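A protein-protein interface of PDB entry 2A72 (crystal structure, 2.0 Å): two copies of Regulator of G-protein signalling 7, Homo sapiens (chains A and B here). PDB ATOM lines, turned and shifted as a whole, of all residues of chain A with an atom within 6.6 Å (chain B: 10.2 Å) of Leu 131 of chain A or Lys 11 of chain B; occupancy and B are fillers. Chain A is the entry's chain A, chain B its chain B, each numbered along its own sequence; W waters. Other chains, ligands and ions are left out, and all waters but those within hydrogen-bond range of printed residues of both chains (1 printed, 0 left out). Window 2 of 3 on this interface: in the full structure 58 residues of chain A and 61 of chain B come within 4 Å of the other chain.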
ATOM      1  N   ILE A 122      28.224  17.352  -3.623  1.00  0.00           N
ATOM      2  CA  ILE A 122      28.304  16.390  -2.517  1.00  0.00           C
ATOM      3  C   ILE A 122      28.351  17.108  -1.141  1.00  0.00           C
ATOM      4  O   ILE A 122      27.728  16.638  -0.190  1.00  0.00           O
ATOM      5  CB  ILE A 122      29.481  15.429  -2.674  1.00  0.00           C
ATOM      6  CG1 ILE A 122      29.348  14.631  -3.995  1.00  0.00           C
ATOM      7  CG2 ILE A 122      29.578  14.442  -1.451  1.00  0.00           C
ATOM      8  CD1 ILE A 122      28.048  13.876  -4.123  1.00  0.00           C
ATOM      9  N   ALA A 126      21.610  20.239   0.048  1.00  0.00           N
ATOM     10  CA  ALA A 126      20.750  19.410  -0.822  1.00  0.00           C
ATOM     11  C   ALA A 126      21.124  17.910  -0.740  1.00  0.00           C
ATOM     12  O   ALA A 126      20.268  17.069  -0.421  1.00  0.00           O
ATOM     13  CB  ALA A 126      20.813  19.902  -2.264  1.00  0.00           C
ATOM     14  N   TYR A 127      22.392  17.576  -0.965  1.00  0.00           N
ATOM     15  CA  TYR A 127      22.810  16.173  -0.872  1.00  0.00           C
ATOM     16  C   TYR A 127      22.839  15.645   0.559  1.00  0.00           C
ATOM     17  O   TYR A 127      22.348  14.559   0.843  1.00  0.00           O
ATOM     18  CB  TYR A 127      24.186  15.954  -1.522  1.00  0.00           C
ATOM     19  CG  TYR A 127      24.613  14.501  -1.532  1.00  0.00           C
ATOM     20  CD1 TYR A 127      23.937  13.566  -2.314  1.00  0.00           C
ATOM     21  CD2 TYR A 127      25.671  14.061  -0.762  1.00  0.00           C
ATOM     22  CE1 TYR A 127      24.304  12.242  -2.321  1.00  0.00           C
ATOM     23  CE2 TYR A 127      26.063  12.719  -0.764  1.00  0.00           C
ATOM     24  CZ  TYR A 127      25.374  11.810  -1.548  1.00  0.00           C
ATOM     25  OH  TYR A 127      25.737  10.476  -1.572  1.00  0.00           O
ATOM     26  N   GLN A 128      23.445  16.413   1.458  1.00  0.00           N
ATOM     27  CA  GLN A 128      23.614  15.987   2.832  1.00  0.00           C
ATOM     28  C   GLN A 128      22.262  15.807   3.500  1.00  0.00           C
ATOM     29  O   GLN A 128      22.097  14.897   4.284  1.00  0.00           O
ATOM     30  CB  GLN A 128      24.504  16.980   3.594  1.00  0.00           C
ATOM     31  CG  GLN A 128      25.962  16.991   3.073  1.00  0.00           C
ATOM     32  CD  GLN A 128      26.682  15.695   3.385  1.00  0.00           C
ATOM     33  OE1 GLN A 128      26.615  15.207   4.500  1.00  0.00           O
ATOM     34  NE2 GLN A 128      27.362  15.130   2.395  1.00  0.00           N
ATOM     35  N   GLU A 129      21.278  16.634   3.146  1.00  0.00           N
ATOM     36  CA  GLU A 129      19.922  16.463   3.679  1.00  0.00           C
ATOM     37  C   GLU A 129      19.281  15.144   3.231  1.00  0.00           C
ATOM     38  O   GLU A 129      18.681  14.446   4.047  1.00  0.00           O
ATOM     39  CB  GLU A 129      19.029  17.667   3.359  1.00  0.00           C
ATOM     40  CG  GLU A 129      19.351  18.870   4.249  1.00  0.00           C
ATOM     41  CD  GLU A 129      18.531  20.116   3.940  1.00  0.00           C
ATOM     42  OE1 GLU A 129      17.887  20.191   2.860  1.00  0.00           O
ATOM     43  OE2 GLU A 129      18.538  21.029   4.803  1.00  0.00           O
ATOM     44  N   LEU A 130      19.433  14.796   1.959  1.00  0.00           N
ATOM     45  CA  LEU A 130      19.003  13.480   1.471  1.00  0.00           C
ATOM     46  C   LEU A 130      19.565  12.361   2.330  1.00  0.00           C
ATOM     47  O   LEU A 130      18.814  11.544   2.857  1.00  0.00           O
ATOM     48  CB  LEU A 130      19.454  13.244   0.042  1.00  0.00           C
ATOM     49  CG  LEU A 130      18.545  13.751  -1.057  1.00  0.00           C
ATOM     50  CD1 LEU A 130      19.141  13.371  -2.401  1.00  0.00           C
ATOM     51  CD2 LEU A 130      17.132  13.186  -0.873  1.00  0.00           C
ATOM     52  N   LEU A 131      20.889  12.335   2.472  1.00  0.00           N
ATOM     53  CA  LEU A 131      21.541  11.304   3.276  1.00  0.00           C
ATOM     54  C   LEU A 131      20.899  11.180   4.654  1.00  0.00           C
ATOM     55  O   LEU A 131      20.374  10.122   4.979  1.00  0.00           O
ATOM     56  CB  LEU A 131      23.039  11.562   3.396  1.00  0.00           C
ATOM     57  CG  LEU A 131      23.818  11.231   2.124  1.00  0.00           C
ATOM     58  CD1 LEU A 131      25.262  11.701   2.299  1.00  0.00           C
ATOM     59  CD2 LEU A 131      23.762   9.744   1.804  1.00  0.00           C
ATOM     60  N   GLN A 132      20.922  12.262   5.437  1.00  0.00           N
ATOM     61  CA  GLN A 132      20.276  12.310   6.758  1.00  0.00           C
ATOM     62  C   GLN A 132      18.815  11.849   6.738  1.00  0.00           C
ATOM     63  O   GLN A 132      18.409  11.029   7.557  1.00  0.00           O
ATOM     64  CB  GLN A 132      20.327  13.739   7.338  1.00  0.00           C
ATOM     65  CG  GLN A 132      21.677  14.148   7.932  1.00  0.00           C
ATOM     66  N   ALA A 133      18.046  12.407   5.802  1.00  0.00           N
ATOM     67  CA  ALA A 133      16.604  12.215   5.724  1.00  0.00           C
ATOM     68  C   ALA A 133      16.116  12.500   4.321  1.00  0.00           C
ATOM     69  O   ALA A 133      15.847  11.579   3.557  1.00  0.00           O
ATOM     70  CB  ALA A 133      15.900  13.137   6.706  1.00  0.00           C
ATOM     71  N   PRO B   5      14.342   6.289  -4.025  1.00  0.00           N
ATOM     72  CA  PRO B   5      15.695   5.720  -4.026  1.00  0.00           C
ATOM     73  C   PRO B   5      16.096   5.251  -2.638  1.00  0.00           C
ATOM     74  O   PRO B   5      15.814   5.927  -1.637  1.00  0.00           O
ATOM     75  CB  PRO B   5      16.585   6.891  -4.463  1.00  0.00           C
ATOM     76  CG  PRO B   5      15.686   7.884  -5.047  1.00  0.00           C
ATOM     77  CD  PRO B   5      14.324   7.688  -4.481  1.00  0.00           C
ATOM     78  N   SER B   6      16.736   4.091  -2.579  1.00  0.00           N
ATOM     79  CA  SER B   6      17.240   3.555  -1.322  1.00  0.00           C
ATOM     80  C   SER B   6      18.400   4.399  -0.783  1.00  0.00           C
ATOM     81  O   SER B   6      18.977   5.233  -1.493  1.00  0.00           O
ATOM     82  CB  SER B   6      17.730   2.132  -1.536  1.00  0.00           C
ATOM     83  OG  SER B   6      18.815   2.118  -2.442  1.00  0.00           O
ATOM     84  N   GLN B   7      18.735   4.168   0.480  1.00  0.00           N
ATOM     85  CA  GLN B   7      19.874   4.824   1.109  1.00  0.00           C
ATOM     86  C   GLN B   7      21.173   4.525   0.359  1.00  0.00           C
ATOM     87  O   GLN B   7      21.963   5.423   0.096  1.00  0.00           O
ATOM     88  CB  GLN B   7      19.979   4.376   2.558  1.00  0.00           C
ATOM     89  CG  GLN B   7      20.798   5.285   3.411  1.00  0.00           C
ATOM     90  CD  GLN B   7      20.852   4.839   4.848  1.00  0.00           C
ATOM     91  OE1 GLN B   7      20.399   3.739   5.200  1.00  0.00           O
ATOM     92  NE2 GLN B   7      21.407   5.691   5.701  1.00  0.00           N
ATOM     93  N   GLN B   8      21.367   3.267  -0.025  1.00  0.00           N
ATOM     94  CA  GLN B   8      22.595   2.865  -0.694  1.00  0.00           C
ATOM     95  C   GLN B   8      22.768   3.495  -2.049  1.00  0.00           C
ATOM     96  O   GLN B   8      23.875   3.899  -2.397  1.00  0.00           O
ATOM     97  CB  GLN B   8      22.695   1.347  -0.861  1.00  0.00           C
ATOM     98  CG  GLN B   8      24.074   0.925  -1.394  1.00  0.00           C
ATOM     99  CD  GLN B   8      25.230   1.617  -0.638  1.00  0.00           C
ATOM    100  OE1 GLN B   8      25.359   1.467   0.584  1.00  0.00           O
ATOM    101  NE2 GLN B   8      26.051   2.400  -1.368  1.00  0.00           N
ATOM    102  N   ARG B   9      21.682   3.539  -2.819  1.00  0.00           N
ATOM    103  CA  ARG B   9      21.668   4.200  -4.113  1.00  0.00           C
ATOM    104  C   ARG B   9      22.090   5.689  -4.025  1.00  0.00           C
ATOM    105  O   ARG B   9      22.842   6.189  -4.874  1.00  0.00           O
ATOM    106  CB  ARG B   9      20.263   4.049  -4.717  1.00  0.00           C
ATOM    107  CG  ARG B   9      20.060   4.763  -6.022  1.00  0.00           C
ATOM    108  CD  ARG B   9      18.688   4.511  -6.577  1.00  0.00           C
ATOM    109  NE  ARG B   9      18.465   5.227  -7.824  1.00  0.00           N
ATOM    110  CZ  ARG B   9      17.305   5.283  -8.462  1.00  0.00           C
ATOM    111  NH1 ARG B   9      16.241   4.690  -7.962  1.00  0.00           N
ATOM    112  NH2 ARG B   9      17.204   5.962  -9.591  1.00  0.00           N
ATOM    113  N   VAL B  10      21.595   6.384  -2.997  1.00  0.00           N
ATOM    114  CA  VAL B  10      21.903   7.783  -2.784  1.00  0.00           C
ATOM    115  C   VAL B  10      23.354   7.952  -2.334  1.00  0.00           C
ATOM    116  O   VAL B  10      24.059   8.844  -2.841  1.00  0.00           O
ATOM    117  CB  VAL B  10      20.947   8.415  -1.756  1.00  0.00           C
ATOM    118  CG1 VAL B  10      21.403   9.838  -1.387  1.00  0.00           C
ATOM    119  CG2 VAL B  10      19.525   8.453  -2.323  1.00  0.00           C
ATOM    120  N   LYS B  11      23.788   7.101  -1.399  1.00  0.00           N
ATOM    121  CA  LYS B  11      25.189   7.084  -0.949  1.00  0.00           C
ATOM    122  C   LYS B  11      26.160   6.875  -2.107  1.00  0.00           C
ATOM    123  O   LYS B  11      27.228   7.468  -2.131  1.00  0.00           O
ATOM    124  CB  LYS B  11      25.444   5.989   0.105  1.00  0.00           C
ATOM    125  CG  LYS B  11      25.029   6.346   1.519  1.00  0.00           C
ATOM    126  CD  LYS B  11      25.317   5.204   2.480  1.00  0.00           C
ATOM    127  CE  LYS B  11      24.918   5.547   3.891  1.00  0.00           C
ATOM    128  NZ  LYS B  11      24.921   4.352   4.814  1.00  0.00           N
ATOM    129  N   ARG B  12      25.777   6.006  -3.043  1.00  0.00           N
ATOM    130  CA  ARG B  12      26.619   5.633  -4.175  1.00  0.00           C
ATOM    131  C   ARG B  12      26.902   6.829  -5.115  1.00  0.00           C
ATOM    132  O   ARG B  12      27.951   6.879  -5.754  1.00  0.00           O
ATOM    133  CB  ARG B  12      25.989   4.434  -4.912  1.00  0.00           C
ATOM    134  CG  ARG B  12      26.794   3.911  -6.096  1.00  0.00           C
ATOM    135  CD  ARG B  12      26.093   2.754  -6.864  1.00  0.00           C
ATOM    136  NE  ARG B  12      25.431   1.792  -5.975  1.00  0.00           N
ATOM    137  CZ  ARG B  12      24.117   1.543  -5.936  1.00  0.00           C
ATOM    138  NH1 ARG B  12      23.258   2.172  -6.749  1.00  0.00           N
ATOM    139  NH2 ARG B  12      23.646   0.648  -5.068  1.00  0.00           N
ATOM    140  N   TRP B  13      26.004   7.816  -5.151  1.00  0.00           N
ATOM    141  CA  TRP B  13      26.258   9.041  -5.904  1.00  0.00           C
ATOM    142  C   TRP B  13      27.463   9.820  -5.401  1.00  0.00           C
ATOM    143  O   TRP B  13      28.035  10.605  -6.158  1.00  0.00           O
ATOM    144  CB  TRP B  13      25.074  10.001  -5.877  1.00  0.00           C
ATOM    145  CG  TRP B  13      23.769   9.455  -6.305  1.00  0.00           C
ATOM    146  CD1 TRP B  13      23.543   8.346  -7.081  1.00  0.00           C
ATOM    147  CD2 TRP B  13      22.487  10.009  -6.008  1.00  0.00           C
ATOM    148  NE1 TRP B  13      22.191   8.177  -7.271  1.00  0.00           N
ATOM    149  CE2 TRP B  13      21.516   9.174  -6.620  1.00  0.00           C
ATOM    150  CE3 TRP B  13      22.055  11.113  -5.260  1.00  0.00           C
ATOM    151  CZ2 TRP B  13      20.139   9.415  -6.520  1.00  0.00           C
ATOM    152  CZ3 TRP B  13      20.666  11.357  -5.165  1.00  0.00           C
ATOM    153  CH2 TRP B  13      19.735  10.497  -5.786  1.00  0.00           C
ATOM    154  N   GLY B  14      27.819   9.634  -4.130  1.00  0.00           N
ATOM    155  CA  GLY B  14      29.002  10.269  -3.556  1.00  0.00           C
ATOM    156  C   GLY B  14      30.294   9.497  -3.765  1.00  0.00           C
ATOM    157  O   GLY B  14      31.353   9.939  -3.296  1.00  0.00           O
ATOM    158  N   PHE B  15      30.224   8.334  -4.425  1.00  0.00           N
ATOM    159  CA  PHE B  15      31.428   7.537  -4.685  1.00  0.00           C
ATOM    160  C   PHE B  15      32.232   8.017  -5.888  1.00  0.00           C
ATOM    161  O   PHE B  15      33.377   7.614  -6.061  1.00  0.00           O
ATOM    162  CB  PHE B  15      31.082   6.055  -4.830  1.00  0.00           C
ATOM    163  CG  PHE B  15      30.549   5.413  -3.569  1.00  0.00           C
ATOM    164  CD1 PHE B  15      30.647   6.040  -2.325  1.00  0.00           C
ATOM    165  CD2 PHE B  15      29.977   4.153  -3.632  1.00  0.00           C
ATOM    166  CE1 PHE B  15      30.155   5.422  -1.172  1.00  0.00           C
ATOM    167  CE2 PHE B  15      29.494   3.521  -2.483  1.00  0.00           C
ATOM    168  CZ  PHE B  15      29.582   4.154  -1.255  1.00  0.00           C
ATOM    169  N   GLY B  16      31.658   8.878  -6.730  1.00  0.00           N
ATOM    170  CA  GLY B  16      32.413   9.472  -7.815  1.00  0.00           C
ATOM    171  C   GLY B  16      31.447  10.116  -8.772  1.00  0.00           C
ATOM    172  O   GLY B  16      30.257   9.815  -8.757  1.00  0.00           O
ATOM    173  N   MET B  17      31.944  11.027  -9.584  1.00  0.00           N
ATOM    174  CA  MET B  17      31.058  11.746 -10.487  1.00  0.00           C
ATOM    175  C   MET B  17      30.370  10.827 -11.509  1.00  0.00           C
ATOM    176  O   MET B  17      29.223  11.043 -11.876  1.00  0.00           O
ATOM    177  CB  MET B  17      31.805  12.896 -11.177  1.00  0.00           C
ATOM    178  CG  MET B  17      30.843  13.894 -11.834  1.00  0.00           C
ATOM    179  SD  MET B  17      31.635  15.288 -12.624  1.00  0.00           S
ATOM    180  CE  MET B  17      32.556  14.497 -13.962  1.00  0.00           C
ATOM    181  N   GLU B  19      29.356   7.811 -11.073  1.00  0.00           N
ATOM    182  CA  GLU B  19      28.252   7.159 -10.366  1.00  0.00           C
ATOM    183  C   GLU B  19      27.047   8.042 -10.346  1.00  0.00           C
ATOM    184  O   GLU B  19      25.926   7.587 -10.554  1.00  0.00           O
ATOM    185  CB  GLU B  19      28.617   6.847  -8.903  1.00  0.00           C
ATOM    186  CG  GLU B  19      29.815   5.963  -8.737  1.00  0.00           C
ATOM    187  CD  GLU B  19      29.520   4.497  -8.977  1.00  0.00           C
ATOM    188  OE1 GLU B  19      28.361   4.157  -9.332  1.00  0.00           O
ATOM    189  OE2 GLU B  19      30.470   3.695  -8.807  1.00  0.00           O
ATOM    190  N   ALA B  20      27.260   9.311 -10.050  1.00  0.00           N
ATOM    191  CA  ALA B  20      26.135  10.244  -9.985  1.00  0.00           C
ATOM    192  C   ALA B  20      25.539  10.441 -11.382  1.00  0.00           C
ATOM    193  O   ALA B  20      24.325  10.547 -11.517  1.00  0.00           O
ATOM    194  CB  ALA B  20      26.560  11.577  -9.409  1.00  0.00           C
ATOM    195  N   ASP B  23      23.369   7.312 -12.846  1.00  0.00           N
ATOM    196  CA  ASP B  23      22.057   7.140 -12.219  1.00  0.00           C
ATOM    197  C   ASP B  23      21.154   8.294 -12.678  1.00  0.00           C
ATOM    198  O   ASP B  23      21.504   9.440 -12.454  1.00  0.00           O
ATOM    199  CB  ASP B  23      22.224   7.142 -10.691  1.00  0.00           C
ATOM    200  CG  ASP B  23      20.930   6.812  -9.956  1.00  0.00           C
ATOM    201  OD1 ASP B  23      19.860   7.308 -10.323  1.00  0.00           O
ATOM    202  OD2 ASP B  23      20.987   6.043  -9.010  1.00  0.00           O
ATOM    203  N   GLY B  26      20.252  10.545  -9.776  1.00  0.00           N
ATOM    204  CA  GLY B  26      21.480  11.200  -9.347  1.00  0.00           C
ATOM    205  C   GLY B  26      21.828  12.352 -10.266  1.00  0.00           C
ATOM    206  O   GLY B  26      22.185  13.454  -9.803  1.00  0.00           O
ATOM    207  N   GLN B  29      19.449  15.230  -9.752  1.00  0.00           N
ATOM    208  CA  GLN B  29      19.702  15.940  -8.503  1.00  0.00           C
ATOM    209  C   GLN B  29      20.959  16.819  -8.598  1.00  0.00           C
ATOM    210  O   GLN B  29      20.980  17.933  -8.080  1.00  0.00           O
ATOM    211  CB  GLN B  29      19.773  14.946  -7.345  1.00  0.00           C
ATOM    212  CG  GLN B  29      18.438  14.239  -7.093  1.00  0.00           C
ATOM    213  CD  GLN B  29      17.359  15.187  -6.649  1.00  0.00           C
ATOM    214  OE1 GLN B  29      17.558  15.958  -5.717  1.00  0.00           O
ATOM    215  NE2 GLN B  29      16.208  15.160  -7.335  1.00  0.00           N
HETATM  216  O   HOH W   1      22.159   7.978   4.651  1.00  0.00           O
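The backbone carbonyl oxygen (O) of Val 10 of chain B sits at hydrogen-bond distance from the side-chain hydroxyl (OH) of Tyr 127 of chain A.
The side-chain hydroxyl (OH) of Tyr 127 of chain A sits at hydrogen-bond distance from the backbone carbonyl oxygen (O) of Lys 11 of chain B (3.4 Å).
The side-chain hydroxyl of Tyr 127 of chain A sits at hydrogen-bond distance from the backbone NH of Gly 14 of chain B (3.4 Å).
O of Ile 122 of chain A is in hydrogen-bond range of NE2 of Gln 128 of chain A (3.0 Å).
The backbone carbonyl oxygen of Arg 9 of chain B sits close to the indole nitrogen of Trp 13 of chain B (3.2 Å).
NE1 of Trp 13 of chain B is in hydrogen-bond range of OD2 of Asp 23 of chain B (3.0 Å).
Among the printed residues, merely in contact across the chains: Leu 131 of chain A with Lys 11 of chain B (3.6 Å), Leu 130 of chain A with Trp 13 of chain B (3.7 Å), Ile 122 of chain A with Gly 14 of chain B (3.8 Å), Ile 122 of chain A with Trp 13 of chain B (3.9 Å), Tyr 127 of chain A with Trp 13 of chain B (3.9 Å) and Leu 131 of chain A with Val 10 of chain B (3.97 Å).
Leu 131 of chain A touches two residues of chain B.
No residue of chain B comes within 4 Å of Gln 128 of chain A.
Leu 130 of chain A touches one residue of chain B.
No residue of chain B comes within 4 Å of Gln 132 of chain A.
No residue of chain B comes within 4 Å of Ala 133 of chain A.
Printed residues of chain B within 4 Å of Tyr 127 of chain A: Val 10 (2.7 Å), Lys 11 (3.4 Å), Trp 13 (3.9 Å) and Gly 14 (3.4 Å).
Printed residues of chain A within 4 Å of Trp 13 of chain B: Ile 122, Tyr 127 and Leu 130.
Printed residues of chain B within 4 Å of Ile 122 of chain A: Trp 13 (3.9 Å) and Gly 14 (3.8 Å).
Glu 19 of chain B touches none of the printed residues of chain A.
The nearest printed residue of chain A that does not touch Lys 11 of chain B is Ile 122 of chain A (6.8 Å).
The nearest printed residue of chain B that does not touch Tyr 127 of chain A is Arg 12 of chain B (4.7 Å).
Along chain B the printed residues that touch a printed residue of chain A span positions 10 to 14.
Among the printed residues, 9 pairs touch across the chains.
Among the printed residues, no Asp or Glu carboxylate lies within 4 Å of a Lys or Arg side-chain nitrogen of the other chain.
No position is printed for both chains.
Of the 9 pairs that touch across the chains among the printed residues, none has its exchanged pair printed and touching as well.
Water W1 bridges NE2 of Gln 7 of chain B and O of Leu 131 of chain A.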
